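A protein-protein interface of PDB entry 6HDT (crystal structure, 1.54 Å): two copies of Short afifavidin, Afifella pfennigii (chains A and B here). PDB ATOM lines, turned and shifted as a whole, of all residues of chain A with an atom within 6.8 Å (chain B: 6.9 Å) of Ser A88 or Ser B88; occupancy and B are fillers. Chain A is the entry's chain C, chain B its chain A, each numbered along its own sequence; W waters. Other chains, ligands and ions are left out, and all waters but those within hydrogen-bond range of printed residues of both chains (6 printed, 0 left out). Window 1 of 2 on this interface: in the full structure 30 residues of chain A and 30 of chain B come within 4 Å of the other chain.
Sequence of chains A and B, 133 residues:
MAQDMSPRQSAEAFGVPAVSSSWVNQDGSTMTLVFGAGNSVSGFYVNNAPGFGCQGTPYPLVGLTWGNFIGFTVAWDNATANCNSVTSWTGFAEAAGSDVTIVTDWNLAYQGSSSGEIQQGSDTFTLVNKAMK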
ATOM      1  N   LEU A  64     -37.139 -19.134 -24.256  1.00  0.00           N
ATOM      2  CA  LEU A  64     -38.044 -18.753 -23.149  1.00  0.00           C
ATOM      3  C   LEU A  64     -38.153 -17.267 -23.023  1.00  0.00           C
ATOM      4  O   LEU A  64     -37.277 -16.540 -23.422  1.00  0.00           O
ATOM      5  CB  LEU A  64     -37.543 -19.304 -21.814  1.00  0.00           C
ATOM      6  CG  LEU A  64     -37.384 -20.826 -21.700  1.00  0.00           C
ATOM      7  CD1 LEU A  64     -36.578 -21.209 -20.469  1.00  0.00           C
ATOM      8  CD2 LEU A  64     -38.724 -21.539 -21.666  1.00  0.00           C
ATOM      9  N   ILE A  70     -36.335 -12.025 -23.519  1.00  0.00           N
ATOM     10  CA  ILE A  70     -36.417 -13.225 -24.302  1.00  0.00           C
ATOM     11  C   ILE A  70     -35.013 -13.758 -24.529  1.00  0.00           C
ATOM     12  O   ILE A  70     -34.076 -13.007 -24.620  1.00  0.00           O
ATOM     13  CB  ILE A  70     -37.091 -12.968 -25.664  1.00  0.00           C
ATOM     14  CG1 ILE A  70     -37.302 -14.263 -26.460  1.00  0.00           C
ATOM     15  CG2 ILE A  70     -36.286 -11.978 -26.503  1.00  0.00           C
ATOM     16  CD1 ILE A  70     -38.380 -14.105 -27.520  1.00  0.00           C
ATOM     17  N   GLY A  71     -34.925 -15.067 -24.627  1.00  0.00           N
ATOM     18  CA  GLY A  71     -33.701 -15.711 -25.082  1.00  0.00           C
ATOM     19  C   GLY A  71     -34.110 -16.807 -26.037  1.00  0.00           C
ATOM     20  O   GLY A  71     -35.076 -17.504 -25.779  1.00  0.00           O
ATOM     21  N   PHE A  72     -33.341 -17.035 -27.105  1.00  0.00           N
ATOM     22  CA  PHE A  72     -33.704 -18.136 -27.996  1.00  0.00           C
ATOM     23  C   PHE A  72     -32.498 -18.612 -28.744  1.00  0.00           C
ATOM     24  O   PHE A  72     -31.522 -17.878 -28.906  1.00  0.00           O
ATOM     25  CB  PHE A  72     -34.911 -17.802 -28.919  1.00  0.00           C
ATOM     26  CG  PHE A  72     -34.682 -16.636 -29.856  1.00  0.00           C
ATOM     27  CD1 PHE A  72     -34.954 -15.334 -29.470  1.00  0.00           C
ATOM     28  CD2 PHE A  72     -34.186 -16.855 -31.133  1.00  0.00           C
ATOM     29  CE1 PHE A  72     -34.746 -14.278 -30.333  1.00  0.00           C
ATOM     30  CE2 PHE A  72     -33.967 -15.806 -31.998  1.00  0.00           C
ATOM     31  CZ  PHE A  72     -34.249 -14.512 -31.600  1.00  0.00           C
ATOM     32  N   THR A  73     -32.599 -19.847 -29.186  1.00  0.00           N
ATOM     33  CA  THR A  73     -31.466 -20.494 -29.852  1.00  0.00           C
ATOM     34  C   THR A  73     -31.901 -21.078 -31.205  1.00  0.00           C
ATOM     35  O   THR A  73     -33.050 -21.517 -31.354  1.00  0.00           O
ATOM     36  CB  THR A  73     -30.947 -21.595 -28.928  1.00  0.00           C
ATOM     37  OG1 THR A  73     -30.509 -21.026 -27.704  1.00  0.00           O
ATOM     38  CG2 THR A  73     -29.729 -22.353 -29.552  1.00  0.00           C
ATOM     39  N   VAL A  74     -30.965 -21.162 -32.157  1.00  0.00           N
ATOM     40  CA  VAL A  74     -31.180 -21.823 -33.454  1.00  0.00           C
ATOM     41  C   VAL A  74     -29.935 -22.682 -33.639  1.00  0.00           C
ATOM     42  O   VAL A  74     -28.839 -22.177 -33.458  1.00  0.00           O
ATOM     43  CB  VAL A  74     -31.222 -20.829 -34.643  1.00  0.00           C
ATOM     44  CG1 VAL A  74     -31.086 -21.508 -35.990  1.00  0.00           C
ATOM     45  CG2 VAL A  74     -32.504 -20.034 -34.639  1.00  0.00           C
ATOM     46  N   TRP A  76     -27.931 -24.560 -36.579  1.00  0.00           N
ATOM     47  CA  TRP A  76     -27.822 -24.404 -38.032  1.00  0.00           C
ATOM     48  C   TRP A  76     -27.691 -25.747 -38.755  1.00  0.00           C
ATOM     49  O   TRP A  76     -26.700 -26.037 -39.446  1.00  0.00           O
ATOM     50  CB  TRP A  76     -26.703 -23.390 -38.375  1.00  0.00           C
ATOM     51  CG  TRP A  76     -26.975 -22.055 -37.714  1.00  0.00           C
ATOM     52  CD1 TRP A  76     -26.347 -21.542 -36.641  1.00  0.00           C
ATOM     53  CD2 TRP A  76     -27.985 -21.090 -38.085  1.00  0.00           C
ATOM     54  NE1 TRP A  76     -26.891 -20.332 -36.299  1.00  0.00           N
ATOM     55  CE2 TRP A  76     -27.880 -20.024 -37.193  1.00  0.00           C
ATOM     56  CE3 TRP A  76     -28.929 -21.025 -39.105  1.00  0.00           C
ATOM     57  CZ2 TRP A  76     -28.736 -18.907 -37.255  1.00  0.00           C
ATOM     58  CZ3 TRP A  76     -29.759 -19.944 -39.173  1.00  0.00           C
ATOM     59  CH2 TRP A  76     -29.649 -18.894 -38.261  1.00  0.00           C
ATOM     60  N   VAL A  86     -24.239 -22.975 -33.824  1.00  0.00           N
ATOM     61  CA  VAL A  86     -25.453 -22.634 -33.089  1.00  0.00           C
ATOM     62  C   VAL A  86     -25.399 -21.161 -32.692  1.00  0.00           C
ATOM     63  O   VAL A  86     -24.357 -20.684 -32.283  1.00  0.00           O
ATOM     64  CB  VAL A  86     -25.553 -23.475 -31.773  1.00  0.00           C
ATOM     65  CG1 VAL A  86     -26.710 -23.033 -30.914  1.00  0.00           C
ATOM     66  CG2 VAL A  86     -25.709 -24.950 -32.062  1.00  0.00           C
ATOM     67  N   THR A  87     -26.540 -20.466 -32.722  1.00  0.00           N
ATOM     68  CA  THR A  87     -26.607 -19.112 -32.287  1.00  0.00           C
ATOM     69  C   THR A  87     -27.654 -18.993 -31.186  1.00  0.00           C
ATOM     70  O   THR A  87     -28.701 -19.647 -31.268  1.00  0.00           O
ATOM     71  CB  THR A  87     -27.023 -18.202 -33.451  1.00  0.00           C
ATOM     72  OG1 THR A  87     -26.058 -18.265 -34.510  1.00  0.00           O
ATOM     73  CG2 THR A  87     -27.198 -16.714 -32.972  1.00  0.00           C
ATOM     74  N   SER A  88     -27.352 -18.208 -30.150  1.00  0.00           N
ATOM     75  CA  SER A  88     -28.399 -17.772 -29.211  1.00  0.00           C
ATOM     76  C   SER A  88     -28.469 -16.257 -29.179  1.00  0.00           C
ATOM     77  O   SER A  88     -27.433 -15.583 -29.176  1.00  0.00           O
ATOM     78  CB  SER A  88     -28.183 -18.287 -27.775  1.00  0.00           C
ATOM     79  OG  SER A  88     -28.115 -19.699 -27.677  1.00  0.00           O
ATOM     80  N   TRP A  89     -29.710 -15.750 -29.118  1.00  0.00           N
ATOM     81  CA  TRP A  89     -30.006 -14.357 -28.952  1.00  0.00           C
ATOM     82  C   TRP A  89     -30.643 -14.125 -27.574  1.00  0.00           C
ATOM     83  O   TRP A  89     -31.462 -14.936 -27.100  1.00  0.00           O
ATOM     84  CB  TRP A  89     -31.084 -13.928 -29.960  1.00  0.00           C
ATOM     85  CG  TRP A  89     -30.695 -13.910 -31.428  1.00  0.00           C
ATOM     86  CD1 TRP A  89     -30.430 -12.796 -32.185  1.00  0.00           C
ATOM     87  CD2 TRP A  89     -30.602 -15.027 -32.326  1.00  0.00           C
ATOM     88  NE1 TRP A  89     -30.196 -13.129 -33.477  1.00  0.00           N
ATOM     89  CE2 TRP A  89     -30.279 -14.494 -33.603  1.00  0.00           C
ATOM     90  CE3 TRP A  89     -30.821 -16.408 -32.202  1.00  0.00           C
ATOM     91  CZ2 TRP A  89     -30.147 -15.289 -34.721  1.00  0.00           C
ATOM     92  CZ3 TRP A  89     -30.631 -17.204 -33.320  1.00  0.00           C
ATOM     93  CH2 TRP A  89     -30.313 -16.639 -34.560  1.00  0.00           C
ATOM     94  N   THR A  90     -30.319 -12.990 -26.966  1.00  0.00           N
ATOM     95  CA  THR A  90     -30.966 -12.610 -25.712  1.00  0.00           C
ATOM     96  C   THR A  90     -31.269 -11.140 -25.782  1.00  0.00           C
ATOM     97  O   THR A  90     -30.428 -10.371 -26.267  1.00  0.00           O
ATOM     98  CB  THR A  90     -30.027 -12.888 -24.514  1.00  0.00           C
ATOM     99  OG1 THR A  90     -29.469 -14.195 -24.644  1.00  0.00           O
ATOM    100  CG2 THR A  90     -30.732 -12.860 -23.239  1.00  0.00           C
ATOM    101  N   GLY A  91     -32.454 -10.714 -25.321  1.00  0.00           N
ATOM    102  CA  GLY A  91     -32.699  -9.273 -25.320  1.00  0.00           C
ATOM    103  C   GLY A  91     -34.053  -8.916 -24.814  1.00  0.00           C
ATOM    104  O   GLY A  91     -34.656  -9.670 -24.063  1.00  0.00           O
ATOM    105  N   ASP A 105     -28.608  -9.133 -28.359  1.00  0.00           N
ATOM    106  CA  ASP A 105     -27.215  -9.478 -28.599  1.00  0.00           C
ATOM    107  C   ASP A 105     -27.191 -10.953 -28.870  1.00  0.00           C
ATOM    108  O   ASP A 105     -27.973 -11.706 -28.297  1.00  0.00           O
ATOM    109  CB  ASP A 105     -26.341  -9.139 -27.381  1.00  0.00           C
ATOM    110  CG  ASP A 105     -26.078  -7.640 -27.231  1.00  0.00           C
ATOM    111  OD1 ASP A 105     -26.145  -6.894 -28.256  1.00  0.00           O
ATOM    112  OD2 ASP A 105     -25.788  -7.210 -26.080  1.00  0.00           O
ATOM    113  N   TRP A 106     -26.264 -11.384 -29.731  1.00  0.00           N
ATOM    114  CA  TRP A 106     -26.186 -12.798 -30.049  1.00  0.00           C
ATOM    115  C   TRP A 106     -24.778 -13.283 -29.999  1.00  0.00           C
ATOM    116  O   TRP A 106     -23.826 -12.523 -30.109  1.00  0.00           O
ATOM    117  CB  TRP A 106     -26.794 -13.129 -31.434  1.00  0.00           C
ATOM    118  CG  TRP A 106     -26.318 -12.311 -32.608  1.00  0.00           C
ATOM    119  CD1 TRP A 106     -26.968 -11.239 -33.176  1.00  0.00           C
ATOM    120  CD2 TRP A 106     -25.129 -12.511 -33.389  1.00  0.00           C
ATOM    121  NE1 TRP A 106     -26.256 -10.750 -34.229  1.00  0.00           N
ATOM    122  CE2 TRP A 106     -25.115 -11.512 -34.389  1.00  0.00           C
ATOM    123  CE3 TRP A 106     -24.078 -13.433 -33.343  1.00  0.00           C
ATOM    124  CZ2 TRP A 106     -24.112 -11.428 -35.344  1.00  0.00           C
ATOM    125  CZ3 TRP A 106     -23.060 -13.326 -34.269  1.00  0.00           C
ATOM    126  CH2 TRP A 106     -23.075 -12.343 -35.250  1.00  0.00           C
ATOM    127  N   ASN A 107     -24.700 -14.589 -29.834  1.00  0.00           N
ATOM    128  CA  ASN A 107     -23.440 -15.315 -29.860  1.00  0.00           C
ATOM    129  C   ASN A 107     -23.658 -16.468 -30.820  1.00  0.00           C
ATOM    130  O   ASN A 107     -24.664 -17.178 -30.720  1.00  0.00           O
ATOM    131  CB  ASN A 107     -23.090 -15.869 -28.486  1.00  0.00           C
ATOM    132  CG  ASN A 107     -22.589 -14.816 -27.520  1.00  0.00           C
ATOM    133  OD1 ASN A 107     -21.789 -13.952 -27.867  1.00  0.00           O
ATOM    134  ND2 ASN A 107     -23.041 -14.912 -26.275  1.00  0.00           N
ATOM    135  N   LEU A 108     -22.655 -16.697 -31.677  1.00  0.00           N
ATOM    136  CA  LEU A 108     -22.648 -17.753 -32.664  1.00  0.00           C
ATOM    137  C   LEU A 108     -21.424 -18.588 -32.366  1.00  0.00           C
ATOM    138  O   LEU A 108     -20.319 -18.075 -32.463  1.00  0.00           O
ATOM    139  CB  LEU A 108     -22.543 -17.166 -34.081  1.00  0.00           C
ATOM    140  CG  LEU A 108     -22.132 -18.072 -35.264  1.00  0.00           C
ATOM    141  CD1 LEU A 108     -23.179 -19.135 -35.494  1.00  0.00           C
ATOM    142  CD2 LEU A 108     -21.941 -17.258 -36.537  1.00  0.00           C
ATOM    143  N   ALA A 109     -21.650 -19.836 -31.971  1.00  0.00           N
ATOM    144  CA  ALA A 109     -20.562 -20.749 -31.689  1.00  0.00           C
ATOM    145  C   ALA A 109     -20.378 -21.636 -32.928  1.00  0.00           C
ATOM    146  O   ALA A 109     -21.349 -22.208 -33.472  1.00  0.00           O
ATOM    147  CB  ALA A 109     -20.873 -21.586 -30.432  1.00  0.00           C
ATOM    148  N   GLY B  63     -32.928 -25.459 -25.004  1.00  0.00           N
ATOM    149  CA  GLY B  63     -31.982 -25.044 -26.015  1.00  0.00           C
ATOM    150  C   GLY B  63     -31.987 -25.981 -27.192  1.00  0.00           C
ATOM    151  O   GLY B  63     -32.895 -26.814 -27.351  1.00  0.00           O
ATOM    152  N   LEU B  64     -30.972 -25.806 -28.028  1.00  0.00           N
ATOM    153  CA  LEU B  64     -30.719 -26.689 -29.152  1.00  0.00           C
ATOM    154  C   LEU B  64     -29.233 -26.961 -29.252  1.00  0.00           C
ATOM    155  O   LEU B  64     -28.408 -26.236 -28.737  1.00  0.00           O
ATOM    156  CB  LEU B  64     -31.194 -26.070 -30.460  1.00  0.00           C
ATOM    157  CG  LEU B  64     -32.699 -25.833 -30.575  1.00  0.00           C
ATOM    158  CD1 LEU B  64     -33.000 -24.844 -31.694  1.00  0.00           C
ATOM    159  CD2 LEU B  64     -33.457 -27.140 -30.727  1.00  0.00           C
ATOM    160  N   ILE B  70     -23.741 -25.829 -28.749  1.00  0.00           N
ATOM    161  CA  ILE B  70     -24.937 -25.759 -27.946  1.00  0.00           C
ATOM    162  C   ILE B  70     -25.329 -24.322 -27.650  1.00  0.00           C
ATOM    163  O   ILE B  70     -24.492 -23.444 -27.578  1.00  0.00           O
ATOM    164  CB  ILE B  70     -24.744 -26.544 -26.641  1.00  0.00           C
ATOM    165  CG1 ILE B  70     -26.094 -26.779 -25.927  1.00  0.00           C
ATOM    166  CG2 ILE B  70     -23.724 -25.882 -25.748  1.00  0.00           C
ATOM    167  CD1 ILE B  70     -26.006 -27.831 -24.827  1.00  0.00           C
ATOM    168  N   GLY B  71     -26.629 -24.126 -27.476  1.00  0.00           N
ATOM    169  CA  GLY B  71     -27.152 -22.865 -26.944  1.00  0.00           C
ATOM    170  C   GLY B  71     -28.355 -23.173 -26.095  1.00  0.00           C
ATOM    171  O   GLY B  71     -29.141 -24.065 -26.434  1.00  0.00           O
ATOM    172  N   PHE B  72     -28.498 -22.443 -24.989  1.00  0.00           N
ATOM    173  CA  PHE B  72     -29.626 -22.674 -24.108  1.00  0.00           C
ATOM    174  C   PHE B  72     -29.975 -21.448 -23.303  1.00  0.00           C
ATOM    175  O   PHE B  72     -29.148 -20.578 -23.052  1.00  0.00           O
ATOM    176  CB  PHE B  72     -29.418 -23.867 -23.175  1.00  0.00           C
ATOM    177  CG  PHE B  72     -28.153 -23.802 -22.355  1.00  0.00           C
ATOM    178  CD1 PHE B  72     -26.969 -24.357 -22.819  1.00  0.00           C
ATOM    179  CD2 PHE B  72     -28.162 -23.246 -21.096  1.00  0.00           C
ATOM    180  CE1 PHE B  72     -25.820 -24.300 -22.057  1.00  0.00           C
ATOM    181  CE2 PHE B  72     -27.016 -23.172 -20.328  1.00  0.00           C
ATOM    182  CZ  PHE B  72     -25.828 -23.724 -20.808  1.00  0.00           C
ATOM    183  N   THR B  73     -31.248 -21.397 -22.930  1.00  0.00           N
ATOM    184  CA  THR B  73     -31.801 -20.240 -22.230  1.00  0.00           C
ATOM    185  C   THR B  73     -32.430 -20.635 -20.908  1.00  0.00           C
ATOM    186  O   THR B  73     -33.010 -21.704 -20.814  1.00  0.00           O
ATOM    187  CB  THR B  73     -32.840 -19.552 -23.113  1.00  0.00           C
ATOM    188  OG1 THR B  73     -32.200 -19.099 -24.295  1.00  0.00           O
ATOM    189  CG2 THR B  73     -33.498 -18.365 -22.420  1.00  0.00           C
ATOM    190  N   VAL B  74     -32.314 -19.763 -19.904  1.00  0.00           N
ATOM    191  CA  VAL B  74     -32.990 -19.906 -18.614  1.00  0.00           C
ATOM    192  C   VAL B  74     -33.726 -18.579 -18.320  1.00  0.00           C
ATOM    193  O   VAL B  74     -33.132 -17.493 -18.306  1.00  0.00           O
ATOM    194  CB  VAL B  74     -32.007 -20.178 -17.469  1.00  0.00           C
ATOM    195  CG1 VAL B  74     -32.702 -20.062 -16.112  1.00  0.00           C
ATOM    196  CG2 VAL B  74     -31.337 -21.522 -17.631  1.00  0.00           C
ATOM    197  N   TRP B  76     -35.515 -16.541 -15.396  1.00  0.00           N
ATOM    198  CA  TRP B  76     -35.324 -16.601 -13.940  1.00  0.00           C
ATOM    199  C   TRP B  76     -36.642 -16.417 -13.188  1.00  0.00           C
ATOM    200  O   TRP B  76     -36.824 -15.439 -12.475  1.00  0.00           O
ATOM    201  CB  TRP B  76     -34.228 -15.624 -13.498  1.00  0.00           C
ATOM    202  CG  TRP B  76     -32.918 -15.989 -14.144  1.00  0.00           C
ATOM    203  CD1 TRP B  76     -32.335 -15.392 -15.201  1.00  0.00           C
ATOM    204  CD2 TRP B  76     -32.076 -17.095 -13.786  1.00  0.00           C
ATOM    205  NE1 TRP B  76     -31.141 -16.069 -15.559  1.00  0.00           N
ATOM    206  CE2 TRP B  76     -30.963 -17.090 -14.671  1.00  0.00           C
ATOM    207  CE3 TRP B  76     -32.115 -18.044 -12.755  1.00  0.00           C
ATOM    208  CZ2 TRP B  76     -29.949 -18.035 -14.587  1.00  0.00           C
ATOM    209  CZ3 TRP B  76     -31.109 -18.990 -12.696  1.00  0.00           C
ATOM    210  CH2 TRP B  76     -30.034 -18.949 -13.581  1.00  0.00           C
ATOM    211  N   VAL B  86     -33.617 -12.961 -18.079  1.00  0.00           N
ATOM    212  CA  VAL B  86     -33.413 -14.159 -18.878  1.00  0.00           C
ATOM    213  C   VAL B  86     -31.952 -14.207 -19.293  1.00  0.00           C
ATOM    214  O   VAL B  86     -31.433 -13.213 -19.759  1.00  0.00           O
ATOM    215  CB  VAL B  86     -34.264 -14.129 -20.167  1.00  0.00           C
ATOM    216  CG1 VAL B  86     -33.952 -15.319 -21.059  1.00  0.00           C
ATOM    217  CG2 VAL B  86     -35.738 -14.050 -19.842  1.00  0.00           C
ATOM    218  N   THR B  87     -31.331 -15.386 -19.204  1.00  0.00           N
ATOM    219  CA  THR B  87     -29.948 -15.596 -19.739  1.00  0.00           C
ATOM    220  C   THR B  87     -29.945 -16.625 -20.868  1.00  0.00           C
ATOM    221  O   THR B  87     -30.688 -17.597 -20.848  1.00  0.00           O
ATOM    222  CB  THR B  87     -29.011 -16.102 -18.612  1.00  0.00           C
ATOM    223  OG1 THR B  87     -29.059 -15.229 -17.484  1.00  0.00           O
ATOM    224  CG2 THR B  87     -27.568 -16.266 -19.041  1.00  0.00           C
ATOM    225  N   SER B  88     -29.081 -16.413 -21.866  1.00  0.00           N
ATOM    226  CA  SER B  88     -28.765 -17.468 -22.828  1.00  0.00           C
ATOM    227  C   SER B  88     -27.275 -17.685 -22.848  1.00  0.00           C
ATOM    228  O   SER B  88     -26.515 -16.755 -22.845  1.00  0.00           O
ATOM    229  CB  SER B  88     -29.252 -17.146 -24.231  1.00  0.00           C
ATOM    230  OG  SER B  88     -30.673 -16.781 -24.244  1.00  0.00           O
ATOM    231  N   TRP B  89     -26.884 -18.950 -22.972  1.00  0.00           N
ATOM    232  CA  TRP B  89     -25.497 -19.304 -23.100  1.00  0.00           C
ATOM    233  C   TRP B  89     -25.314 -19.896 -24.477  1.00  0.00           C
ATOM    234  O   TRP B  89     -26.210 -20.569 -24.977  1.00  0.00           O
ATOM    235  CB  TRP B  89     -25.139 -20.397 -22.098  1.00  0.00           C
ATOM    236  CG  TRP B  89     -25.039 -20.033 -20.668  1.00  0.00           C
ATOM    237  CD1 TRP B  89     -23.901 -19.855 -19.946  1.00  0.00           C
ATOM    238  CD2 TRP B  89     -26.122 -19.871 -19.761  1.00  0.00           C
ATOM    239  NE1 TRP B  89     -24.205 -19.568 -18.648  1.00  0.00           N
ATOM    240  CE2 TRP B  89     -25.567 -19.574 -18.503  1.00  0.00           C
ATOM    241  CE3 TRP B  89     -27.515 -19.959 -19.886  1.00  0.00           C
ATOM    242  CZ2 TRP B  89     -26.349 -19.380 -17.374  1.00  0.00           C
ATOM    243  CZ3 TRP B  89     -28.298 -19.740 -18.749  1.00  0.00           C
ATOM    244  CH2 TRP B  89     -27.720 -19.452 -17.527  1.00  0.00           C
ATOM    245  N   THR B  90     -24.125 -19.737 -25.062  1.00  0.00           N
ATOM    246  CA  THR B  90     -23.828 -20.378 -26.339  1.00  0.00           C
ATOM    247  C   THR B  90     -22.370 -20.772 -26.341  1.00  0.00           C
ATOM    248  O   THR B  90     -21.543 -20.041 -25.851  1.00  0.00           O
ATOM    249  CB  THR B  90     -24.130 -19.462 -27.543  1.00  0.00           C
ATOM    250  OG1 THR B  90     -25.341 -18.710 -27.301  1.00  0.00           O
ATOM    251  CG2 THR B  90     -24.251 -20.276 -28.852  1.00  0.00           C
ATOM    252  N   GLY B  91     -22.068 -21.948 -26.854  1.00  0.00           N
ATOM    253  CA  GLY B  91     -20.689 -22.415 -26.735  1.00  0.00           C
ATOM    254  C   GLY B  91     -20.463 -23.746 -27.388  1.00  0.00           C
ATOM    255  O   GLY B  91     -21.249 -24.225 -28.173  1.00  0.00           O
ATOM    256  N   ASP B 105     -20.187 -18.290 -23.830  1.00  0.00           N
ATOM    257  CA  ASP B 105     -20.442 -16.870 -23.540  1.00  0.00           C
ATOM    258  C   ASP B 105     -21.933 -16.723 -23.272  1.00  0.00           C
ATOM    259  O   ASP B 105     -22.745 -17.484 -23.776  1.00  0.00           O
ATOM    260  CB  ASP B 105     -20.069 -15.968 -24.729  1.00  0.00           C
ATOM    261  CG  ASP B 105     -18.562 -15.886 -24.987  1.00  0.00           C
ATOM    262  OD1 ASP B 105     -17.780 -16.128 -24.047  1.00  0.00           O
ATOM    263  OD2 ASP B 105     -18.172 -15.489 -26.112  1.00  0.00           O
ATOM    264  N   TRP B 106     -22.297 -15.751 -22.452  1.00  0.00           N
ATOM    265  CA  TRP B 106     -23.705 -15.598 -22.110  1.00  0.00           C
ATOM    266  C   TRP B 106     -24.071 -14.170 -22.119  1.00  0.00           C
ATOM    267  O   TRP B 106     -23.220 -13.299 -21.917  1.00  0.00           O
ATOM    268  CB  TRP B 106     -24.044 -16.211 -20.742  1.00  0.00           C
ATOM    269  CG  TRP B 106     -23.208 -15.774 -19.545  1.00  0.00           C
ATOM    270  CD1 TRP B 106     -22.168 -16.478 -18.968  1.00  0.00           C
ATOM    271  CD2 TRP B 106     -23.355 -14.572 -18.756  1.00  0.00           C
ATOM    272  NE1 TRP B 106     -21.658 -15.789 -17.913  1.00  0.00           N
ATOM    273  CE2 TRP B 106     -22.377 -14.628 -17.738  1.00  0.00           C
ATOM    274  CE3 TRP B 106     -24.240 -13.462 -18.789  1.00  0.00           C
ATOM    275  CZ2 TRP B 106     -22.217 -13.626 -16.800  1.00  0.00           C
ATOM    276  CZ3 TRP B 106     -24.077 -12.459 -17.830  1.00  0.00           C
ATOM    277  CH2 TRP B 106     -23.079 -12.550 -16.857  1.00  0.00           C
ATOM    278  N   ASN B 107     -25.355 -13.966 -22.385  1.00  0.00           N
ATOM    279  CA  ASN B 107     -25.983 -12.669 -22.271  1.00  0.00           C
ATOM    280  C   ASN B 107     -27.158 -12.792 -21.330  1.00  0.00           C
ATOM    281  O   ASN B 107     -27.837 -13.794 -21.365  1.00  0.00           O
ATOM    282  CB  ASN B 107     -26.504 -12.250 -23.641  1.00  0.00           C
ATOM    283  CG  ASN B 107     -25.405 -11.845 -24.604  1.00  0.00           C
ATOM    284  OD1 ASN B 107     -24.517 -11.067 -24.265  1.00  0.00           O
ATOM    285  ND2 ASN B 107     -25.458 -12.395 -25.806  1.00  0.00           N
ATOM    286  N   LEU B 108     -27.438 -11.730 -20.556  1.00  0.00           N
ATOM    287  CA  LEU B 108     -28.485 -11.718 -19.556  1.00  0.00           C
ATOM    288  C   LEU B 108     -29.267 -10.425 -19.700  1.00  0.00           C
ATOM    289  O   LEU B 108     -28.719  -9.350 -19.457  1.00  0.00           O
ATOM    290  CB  LEU B 108     -27.853 -11.748 -18.181  1.00  0.00           C
ATOM    291  CG  LEU B 108     -28.700 -11.844 -16.909  1.00  0.00           C
ATOM    292  CD1 LEU B 108     -27.759 -12.212 -15.781  1.00  0.00           C
ATOM    293  CD2 LEU B 108     -29.455 -10.565 -16.558  1.00  0.00           C
ATOM    294  N   ALA B 109     -30.515 -10.547 -20.117  1.00  0.00           N
ATOM    295  CA  ALA B 109     -31.439  -9.405 -20.247  1.00  0.00           C
ATOM    296  C   ALA B 109     -32.103  -9.133 -18.922  1.00  0.00           C
ATOM    297  O   ALA B 109     -32.653 -10.056 -18.304  1.00  0.00           O
ATOM    298  CB  ALA B 109     -32.467  -9.713 -21.312  1.00  0.00           C
HETATM  299  O   HOH W   1     -23.056 -11.655 -27.357  1.00  0.00           O
HETATM  300  O   HOH W   2     -32.573 -21.174 -26.010  1.00  0.00           O
HETATM  301  O   HOH W   3     -27.300 -14.633 -26.480  1.00  0.00           O
HETATM  302  O   HOH W   4     -25.490 -16.615 -25.656  1.00  0.00           O
HETATM  303  O   HOH W   5     -23.299  -8.636 -25.006  1.00  0.00           O
HETATM  304  O   HOH W   6     -22.092 -12.687 -24.445  1.00  0.00           O
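Of the 19 printed residues of chain B, 14 touch a printed residue of chain A.
Hydrophobic or aromatic side chains of chain A that line the printed part of chain B: Leu A64, Val A86 and Ala A109.
Among the printed residues, 32 pairs touch across the chains.
Among the printed residues, no Asp or Glu carboxylate lies within 4 Å of a Lys or Arg side-chain nitrogen of the other chain.
Ser A88 touches five residues of chain B.
Ser B88 touches five residues of chain A.
Printed residues of chain B within 4 Å of Asp A105: Asn B107.
Of the printed residues of chain A, Ala B109 touches Thr A90 (3.9 Å) and Gly A91 (3.5 Å).
Of the printed residues of chain A, Leu B64 touches Thr A73 (3.3 Å) and Val A74 (3.9 Å).
Of the printed residues of chain B, Gly A91 touches Ala B109.
Of the printed residues of chain B, Ile A70 touches Val B86.
The nearest printed residue of chain A that does not touch Ile B70 is Ala A109 (5.0 Å).
The side-chain hydroxyl (OG) of Ser B88 lies within hydrogen-bond range of the backbone carbonyl oxygen (O) of Trp A89 (3.5 Å).
The side-chain hydroxyl (OG1) of Thr A90 sits at hydrogen-bond distance from the side-chain hydroxyl (OG) of Ser B88.
The side-chain hydroxyl of Ser A88 is in hydrogen-bond range of the backbone carbonyl oxygen of Trp B89 (3.4 Å).
OG1 of Thr B90 lies close to OG of Ser A88.
Water W1 lies within hydrogen-bond range of OD1 of Asn A107 (2.7 Å), ND2 of Asn B107 (3.0 Å) and O of Trp A106 (3.0 Å).
Water W2 bridges the side-chain hydroxyl (OG1) of Thr A73 (2.7 Å) and the side-chain hydroxyl (OG1) of Thr B73 (2.7 Å).
Water W5 bridges OD1 of Asn B107 (2.8 Å) and OD2 of Asp A105 (3.1 Å).
Water W3 lies within hydrogen-bond range of O of Ser A88 (2.9 Å), OG1 of Thr A90 (2.9 Å) and ND2 of Asn B107 (3.0 Å).
The backbone NH (N) of Leu B64 is in hydrogen-bond range of the backbone carbonyl oxygen (O) of Gly B71, 3.0 Å away.
The side-chain hydroxyl (OG) of Ser B88 sits at hydrogen-bond distance from the side-chain hydroxyl (OG1) of Thr B73.
OG1 of Thr A73 sits at hydrogen-bond distance from OG of Ser A88 (2.7 Å).
The backbone carbonyl oxygen (O) of Thr A87 is in hydrogen-bond range of the backbone NH (N) of Val A74 (2.9 Å).
Ser A88 touches Trp B89, and with the chains exchanged Trp A89 touches Ser B88.
Thr A90 touches Asn B107, and with the chains exchanged Asn A107 touches Thr B90.
Gly A91 touches Ala B109, and with the chains exchanged Ala A109 touches Gly B91.
Asn A107 touches its own counterpart, Asn B107.
Of the 32 pairs that touch across the chains among the printed residues, 30 have their exchanged pair printed and touching as well.
Thr B73 touches Gly A71 (OG1 to C, 3.5 Å).
N of Gly A71 touches CG1 of Val B86, 3.7 Å away.
Ser B88 touches Phe A72 (OG to N, 3.9 Å).
Leu B64 touches Thr A73 (CD1 to O, 3.3 Å).
OG1 of Thr A73 touches C of Gly B71, at 3.4 Å.
Ile B70 touches Val A86.
Phe B72 touches Ser A88 (N to OG, 3.9 Å).
CG2 of Thr A90 touches O of Asn B107 (3.6 Å).
O of Gly A91 touches CB of Ala B109, at 3.5 Å.
CG2 of Thr B90 touches CB of Ala A109, at 3.95 Å.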
